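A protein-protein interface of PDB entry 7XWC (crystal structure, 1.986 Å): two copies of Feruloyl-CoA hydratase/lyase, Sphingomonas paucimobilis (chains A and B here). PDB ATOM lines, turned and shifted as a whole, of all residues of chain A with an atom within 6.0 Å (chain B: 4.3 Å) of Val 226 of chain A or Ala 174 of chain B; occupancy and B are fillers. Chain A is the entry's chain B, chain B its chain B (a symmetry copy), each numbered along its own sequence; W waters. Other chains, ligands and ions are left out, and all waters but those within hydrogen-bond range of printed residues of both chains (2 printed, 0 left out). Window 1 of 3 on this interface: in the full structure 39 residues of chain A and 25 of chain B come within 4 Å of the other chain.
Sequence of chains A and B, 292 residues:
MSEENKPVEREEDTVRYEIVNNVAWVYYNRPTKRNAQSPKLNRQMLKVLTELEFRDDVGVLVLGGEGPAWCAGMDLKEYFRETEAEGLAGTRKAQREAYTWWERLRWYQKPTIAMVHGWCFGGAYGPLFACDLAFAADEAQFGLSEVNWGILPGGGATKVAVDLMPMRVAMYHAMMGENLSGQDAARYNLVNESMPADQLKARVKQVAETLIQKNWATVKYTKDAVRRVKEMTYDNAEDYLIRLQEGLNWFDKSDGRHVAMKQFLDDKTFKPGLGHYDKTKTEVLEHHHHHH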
ATOM      1  N   TYR A 221     -16.211  23.495  13.614  1.00  0.00           N
ATOM      2  CA  TYR A 221     -14.964  24.286  13.571  1.00  0.00           C
ATOM      3  C   TYR A 221     -14.970  25.171  12.310  1.00  0.00           C
ATOM      4  O   TYR A 221     -14.587  26.350  12.403  1.00  0.00           O
ATOM      5  CB  TYR A 221     -13.745  23.381  13.675  1.00  0.00           C
ATOM      6  CG  TYR A 221     -13.332  23.120  15.088  1.00  0.00           C
ATOM      7  CD1 TYR A 221     -13.930  22.114  15.840  1.00  0.00           C
ATOM      8  CD2 TYR A 221     -12.393  23.921  15.706  1.00  0.00           C
ATOM      9  CE1 TYR A 221     -13.579  21.908  17.169  1.00  0.00           C
ATOM     10  CE2 TYR A 221     -12.015  23.709  17.022  1.00  0.00           C
ATOM     11  CZ  TYR A 221     -12.582  22.681  17.742  1.00  0.00           C
ATOM     12  OH  TYR A 221     -12.209  22.489  19.039  1.00  0.00           O
ATOM     13  N   THR A 222     -15.439  24.645  11.181  1.00  0.00           N
ATOM     14  CA  THR A 222     -15.393  25.333   9.885  1.00  0.00           C
ATOM     15  C   THR A 222     -16.408  26.481   9.895  1.00  0.00           C
ATOM     16  O   THR A 222     -16.056  27.570   9.395  1.00  0.00           O
ATOM     17  CB  THR A 222     -15.492  24.330   8.726  1.00  0.00           C
ATOM     18  OG1 THR A 222     -14.518  24.712   7.763  1.00  0.00           O
ATOM     19  CG2 THR A 222     -16.809  24.337   8.003  1.00  0.00           C
ATOM     20  N   LYS A 223     -17.611  26.301  10.451  1.00  0.00           N
ATOM     21  CA  LYS A 223     -18.616  27.392  10.465  1.00  0.00           C
ATOM     22  C   LYS A 223     -18.194  28.469  11.484  1.00  0.00           C
ATOM     23  O   LYS A 223     -18.343  29.676  11.187  1.00  0.00           O
ATOM     24  CB  LYS A 223     -20.030  26.869  10.726  1.00  0.00           C
ATOM     25  CG  LYS A 223     -20.323  26.447  12.161  1.00  0.00           C
ATOM     26  CD  LYS A 223     -21.522  25.506  12.289  1.00  0.00           C
ATOM     27  CE  LYS A 223     -22.140  25.480  13.681  1.00  0.00           C
ATOM     28  NZ  LYS A 223     -23.023  26.651  13.908  1.00  0.00           N
ATOM     29  N   ASP A 224     -17.659  28.080  12.631  1.00  0.00           N
ATOM     30  CA  ASP A 224     -17.185  29.089  13.619  1.00  0.00           C
ATOM     31  C   ASP A 224     -16.036  29.918  12.995  1.00  0.00           C
ATOM     32  O   ASP A 224     -15.890  31.149  13.322  1.00  0.00           O
ATOM     33  CB  ASP A 224     -16.715  28.461  14.948  1.00  0.00           C
ATOM     34  CG  ASP A 224     -17.797  28.161  15.974  1.00  0.00           C
ATOM     35  OD1 ASP A 224     -19.037  28.124  15.601  1.00  0.00           O
ATOM     36  OD2 ASP A 224     -17.408  27.936  17.177  1.00  0.00           O
ATOM     37  N   ALA A 225     -15.203  29.280  12.180  1.00  0.00           N
ATOM     38  CA  ALA A 225     -14.011  29.947  11.609  1.00  0.00           C
ATOM     39  C   ALA A 225     -14.485  31.033  10.636  1.00  0.00           C
ATOM     40  O   ALA A 225     -13.978  32.153  10.709  1.00  0.00           O
ATOM     41  CB  ALA A 225     -13.088  28.930  10.964  1.00  0.00           C
ATOM     42  N   VAL A 226     -15.479  30.754   9.796  1.00  0.00           N
ATOM     43  CA  VAL A 226     -16.013  31.787   8.877  1.00  0.00           C
ATOM     44  C   VAL A 226     -16.455  33.027   9.688  1.00  0.00           C
ATOM     45  O   VAL A 226     -16.163  34.153   9.205  1.00  0.00           O
ATOM     46  CB  VAL A 226     -17.143  31.218   8.004  1.00  0.00           C
ATOM     47  CG1 VAL A 226     -17.814  32.303   7.189  1.00  0.00           C
ATOM     48  CG2 VAL A 226     -16.639  30.095   7.114  1.00  0.00           C
ATOM     49  N   ARG A 227     -17.185  32.846  10.802  1.00  0.00           N
ATOM     50  CA  ARG A 227     -17.842  33.927  11.589  1.00  0.00           C
ATOM     51  C   ARG A 227     -16.725  34.734  12.261  1.00  0.00           C
ATOM     52  O   ARG A 227     -16.787  35.923  12.243  1.00  0.00           O
ATOM     53  CB  ARG A 227     -18.786  33.372  12.666  1.00  0.00           C
ATOM     54  CG  ARG A 227     -20.073  32.774  12.123  1.00  0.00           C
ATOM     55  CD  ARG A 227     -21.022  32.315  13.216  1.00  0.00           C
ATOM     56  NE  ARG A 227     -22.276  31.830  12.661  1.00  0.00           N
ATOM     57  CZ  ARG A 227     -23.285  32.571  12.273  1.00  0.00           C
ATOM     58  NH1 ARG A 227     -23.203  33.883  12.323  1.00  0.00           N
ATOM     59  NH2 ARG A 227     -24.352  31.980  11.749  1.00  0.00           N
ATOM     60  N   ARG A 228     -15.734  34.034  12.785  1.00  0.00           N
ATOM     61  CA  ARG A 228     -14.633  34.605  13.574  1.00  0.00           C
ATOM     62  C   ARG A 228     -13.670  35.390  12.667  1.00  0.00           C
ATOM     63  O   ARG A 228     -13.287  36.508  13.067  1.00  0.00           O
ATOM     64  CB  ARG A 228     -13.909  33.478  14.329  1.00  0.00           C
ATOM     65  CG  ARG A 228     -14.664  32.913  15.518  1.00  0.00           C
ATOM     66  CD  ARG A 228     -14.649  33.793  16.771  1.00  0.00           C
ATOM     67  NE  ARG A 228     -15.518  33.199  17.795  1.00  0.00           N
ATOM     68  CZ  ARG A 228     -16.028  33.821  18.878  1.00  0.00           C
ATOM     69  NH1 ARG A 228     -15.779  35.087  19.140  1.00  0.00           N
ATOM     70  NH2 ARG A 228     -16.865  33.176  19.666  1.00  0.00           N
ATOM     71  N   VAL A 229     -13.242  34.865  11.514  1.00  0.00           N
ATOM     72  CA  VAL A 229     -12.151  35.514  10.722  1.00  0.00           C
ATOM     73  C   VAL A 229     -12.685  36.766  10.022  1.00  0.00           C
ATOM     74  O   VAL A 229     -11.878  37.637   9.688  1.00  0.00           O
ATOM     75  CB  VAL A 229     -11.425  34.584   9.733  1.00  0.00           C
ATOM     76  CG1 VAL A 229     -10.802  33.436  10.488  1.00  0.00           C
ATOM     77  CG2 VAL A 229     -12.303  34.093   8.621  1.00  0.00           C
ATOM     78  N   LYS A 230     -13.997  36.897   9.926  1.00  0.00           N
ATOM     79  CA  LYS A 230     -14.644  38.173   9.563  1.00  0.00           C
ATOM     80  C   LYS A 230     -14.156  39.333  10.446  1.00  0.00           C
ATOM     81  O   LYS A 230     -14.156  40.441   9.952  1.00  0.00           O
ATOM     82  CB  LYS A 230     -16.160  38.032   9.640  1.00  0.00           C
ATOM     83  CG  LYS A 230     -16.903  39.312   9.280  1.00  0.00           C
ATOM     84  CD  LYS A 230     -16.864  39.583   7.815  1.00  0.00           C
ATOM     85  CE  LYS A 230     -18.025  38.895   7.119  1.00  0.00           C
ATOM     86  NZ  LYS A 230     -19.296  39.590   7.449  1.00  0.00           N
ATOM     87  N   VAL B 147     -13.691  20.081   4.188  1.00  0.00           N
ATOM     88  CA  VAL B 147     -14.719  19.656   5.170  1.00  0.00           C
ATOM     89  C   VAL B 147     -14.989  18.143   4.989  1.00  0.00           C
ATOM     90  O   VAL B 147     -15.221  17.448   5.975  1.00  0.00           O
ATOM     91  CB  VAL B 147     -15.971  20.531   5.036  1.00  0.00           C
ATOM     92  CG1 VAL B 147     -16.695  20.387   3.686  1.00  0.00           C
ATOM     93  CG2 VAL B 147     -16.899  20.308   6.195  1.00  0.00           C
ATOM     94  N   THR B 158     -10.153  29.971   4.466  1.00  0.00           N
ATOM     95  CA  THR B 158     -11.371  30.481   5.129  1.00  0.00           C
ATOM     96  C   THR B 158     -11.337  32.012   5.070  1.00  0.00           C
ATOM     97  O   THR B 158     -12.365  32.639   4.754  1.00  0.00           O
ATOM     98  CB  THR B 158     -11.509  29.920   6.556  1.00  0.00           C
ATOM     99  OG1 THR B 158     -11.528  28.494   6.521  1.00  0.00           O
ATOM    100  CG2 THR B 158     -12.745  30.409   7.266  1.00  0.00           C
ATOM    101  N   VAL B 162     -13.835  34.681   3.012  1.00  0.00           N
ATOM    102  CA  VAL B 162     -14.502  35.770   3.771  1.00  0.00           C
ATOM    103  C   VAL B 162     -14.100  37.164   3.273  1.00  0.00           C
ATOM    104  O   VAL B 162     -14.960  38.077   3.346  1.00  0.00           O
ATOM    105  CB  VAL B 162     -14.220  35.567   5.268  1.00  0.00           C
ATOM    106  CG1 VAL B 162     -14.455  36.825   6.083  1.00  0.00           C
ATOM    107  CG2 VAL B 162     -15.070  34.429   5.775  1.00  0.00           C
ATOM    108  N   ALA B 170     -19.495  32.525   1.539  1.00  0.00           N
ATOM    109  CA  ALA B 170     -18.273  31.952   2.126  1.00  0.00           C
ATOM    110  C   ALA B 170     -18.699  30.811   3.036  1.00  0.00           C
ATOM    111  O   ALA B 170     -18.060  29.796   3.035  1.00  0.00           O
ATOM    112  CB  ALA B 170     -17.469  32.970   2.900  1.00  0.00           C
ATOM    113  N   MET B 171     -19.757  31.003   3.791  1.00  0.00           N
ATOM    114  CA  MET B 171     -20.227  29.998   4.784  1.00  0.00           C
ATOM    115  C   MET B 171     -20.623  28.698   4.055  1.00  0.00           C
ATOM    116  O   MET B 171     -20.179  27.649   4.459  1.00  0.00           O
ATOM    117  CB  MET B 171     -21.417  30.563   5.553  1.00  0.00           C
ATOM    118  CG  MET B 171     -21.889  29.661   6.686  1.00  0.00           C
ATOM    119  SD  MET B 171     -20.684  29.432   8.028  1.00  0.00           S
ATOM    120  CE  MET B 171     -20.987  30.896   8.999  1.00  0.00           C
ATOM    121  N   TYR B 172     -21.430  28.784   3.003  1.00  0.00           N
ATOM    122  CA  TYR B 172     -21.856  27.616   2.202  1.00  0.00           C
ATOM    123  C   TYR B 172     -20.622  26.925   1.625  1.00  0.00           C
ATOM    124  O   TYR B 172     -20.474  25.687   1.728  1.00  0.00           O
ATOM    125  CB  TYR B 172     -22.870  28.062   1.145  1.00  0.00           C
ATOM    126  CG  TYR B 172     -23.491  26.921   0.384  1.00  0.00           C
ATOM    127  CD1 TYR B 172     -22.831  26.335  -0.672  1.00  0.00           C
ATOM    128  CD2 TYR B 172     -24.753  26.452   0.700  1.00  0.00           C
ATOM    129  CE1 TYR B 172     -23.406  25.289  -1.395  1.00  0.00           C
ATOM    130  CE2 TYR B 172     -25.342  25.407   0.004  1.00  0.00           C
ATOM    131  CZ  TYR B 172     -24.654  24.817  -1.044  1.00  0.00           C
ATOM    132  OH  TYR B 172     -25.197  23.769  -1.727  1.00  0.00           O
ATOM    133  N   HIS B 173     -19.711  27.723   1.089  1.00  0.00           N
ATOM    134  CA  HIS B 173     -18.491  27.261   0.403  1.00  0.00           C
ATOM    135  C   HIS B 173     -17.676  26.373   1.341  1.00  0.00           C
ATOM    136  O   HIS B 173     -17.270  25.255   0.967  1.00  0.00           O
ATOM    137  CB  HIS B 173     -17.718  28.473  -0.103  1.00  0.00           C
ATOM    138  CG  HIS B 173     -16.779  28.158  -1.204  1.00  0.00           C
ATOM    139  ND1 HIS B 173     -17.200  27.599  -2.400  1.00  0.00           N
ATOM    140  CD2 HIS B 173     -15.432  28.338  -1.291  1.00  0.00           C
ATOM    141  CE1 HIS B 173     -16.141  27.436  -3.163  1.00  0.00           C
ATOM    142  NE2 HIS B 173     -15.049  27.907  -2.509  1.00  0.00           N
ATOM    143  N   ALA B 174     -17.444  26.860   2.541  1.00  0.00           N
ATOM    144  CA  ALA B 174     -16.661  26.148   3.551  1.00  0.00           C
ATOM    145  C   ALA B 174     -17.407  24.915   4.100  1.00  0.00           C
ATOM    146  O   ALA B 174     -16.739  23.901   4.428  1.00  0.00           O
ATOM    147  CB  ALA B 174     -16.375  27.160   4.621  1.00  0.00           C
ATOM    148  N   MET B 175     -18.726  25.022   4.310  1.00  0.00           N
ATOM    149  CA  MET B 175     -19.486  24.021   5.102  1.00  0.00           C
ATOM    150  C   MET B 175     -19.886  22.852   4.204  1.00  0.00           C
ATOM    151  O   MET B 175     -19.901  21.740   4.677  1.00  0.00           O
ATOM    152  CB  MET B 175     -20.762  24.618   5.675  1.00  0.00           C
ATOM    153  CG  MET B 175     -20.519  25.526   6.873  1.00  0.00           C
ATOM    154  SD  MET B 175     -22.107  26.127   7.562  1.00  0.00           S
ATOM    155  CE  MET B 175     -22.897  24.565   7.943  1.00  0.00           C
ATOM    156  N   MET B 176     -20.188  23.121   2.948  1.00  0.00           N
ATOM    157  CA  MET B 176     -20.762  22.103   2.038  1.00  0.00           C
ATOM    158  C   MET B 176     -19.672  21.503   1.147  1.00  0.00           C
ATOM    159  O   MET B 176     -19.881  20.409   0.678  1.00  0.00           O
ATOM    160  CB  MET B 176     -21.882  22.732   1.216  1.00  0.00           C
ATOM    161  CG  MET B 176     -23.056  23.166   2.080  1.00  0.00           C
ATOM    162  SD  MET B 176     -23.955  21.744   2.795  1.00  0.00           S
ATOM    163  CE  MET B 176     -24.785  21.222   1.291  1.00  0.00           C
ATOM    164  N   GLY B 177     -18.543  22.190   0.946  1.00  0.00           N
ATOM    165  CA  GLY B 177     -17.388  21.689   0.179  1.00  0.00           C
ATOM    166  C   GLY B 177     -17.685  21.475  -1.308  1.00  0.00           C
ATOM    167  O   GLY B 177     -16.995  20.664  -1.907  1.00  0.00           O
HETATM  168  O   HOH W   1     -13.758  27.466   7.579  1.00  0.00           O
HETATM  169  O   HOH W   2     -13.556  22.582   6.231  1.00  0.00           O
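Printed residues of chain B that touch a printed residue of chain A: Thr 158, Val 162, Met 171, Ala 174 and Met 175.
Hydrophobic or aromatic side chains of chain B within 4 Å of the printed part of chain A: Val 162, Met 171, Ala 174 and Met 175.
Of the 10 printed residues of chain A, 7 touch a printed residue of chain B.
Printed residues of chain A that touch a printed residue of chain B: Thr 222, Lys 223, Ala 225, Val 226, Arg 227, Val 229 and Lys 230.
Among the printed residues, 13 pairs touch across the chains.
Among the printed residues, no Asp or Glu carboxylate lies within 4 Å of a Lys or Arg side-chain nitrogen of the other chain.
CA of Met 175 of chain B touches CG2 of Thr 222 of chain A, at 3.96 Å.
CE of Met 171 of chain B touches O of Lys 223 of chain A, 3.6 Å away.
Lys 223 of chain A touches Met 175 of chain B (CB to SD, 3.9 Å).
Ala 225 of chain A touches Thr 158 of chain B.
Thr 158 of chain B touches Val 226 of chain A (CG2 to N, 3.7 Å).
Val 226 of chain A touches Val 162 of chain B.
CE of Met 171 of chain B touches CG1 of Val 226 of chain A (3.9 Å).
Thr 158 of chain B touches Val 229 of chain A (CG2 to CG2, 3.95 Å).
Val 162 of chain B touches Val 229 of chain A.
Val 162 of chain B touches Lys 230 of chain A (CG1 to CA, 3.7 Å).
No position is printed for both chains.
Water W1 lies within hydrogen-bond range of OG1 of Thr 158 of chain B (2.7 Å) and OG1 of Thr 222 of chain A (2.9 Å).
Water W2 bridges the side-chain hydroxyl of Thr 222 of chain A (2.8 Å) and the backbone NH of Val 147 of chain B (3.2 Å).
Of chain B, only Thr 158, Val 162, Met 171 and Ala 174 come within 4 Å of Val 226 of chain A.
Of the printed residues of chain B, Arg 227 of chain A touches Met 171 (3.8 Å).
Printed residues of chain B within 4 Å of Lys 230 of chain A: Val 162 (3.7 Å).
Of the printed residues of chain A, Thr 158 of chain B touches Ala 225, Val 226 and Val 229.
Of the printed residues of chain A, Val 162 of chain B touches Val 226, Val 229 and Lys 230.
Ala 170 of chain B touches none of the printed residues of chain A.
Printed residues of chain A within 4 Å of Met 171 of chain B: Lys 223, Val 226 and Arg 227.
Of chain A, only Thr 222 and Val 226 come within 4 Å of Ala 174 of chain B.
Gly 177 of chain B touches none of the printed residues of chain A.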
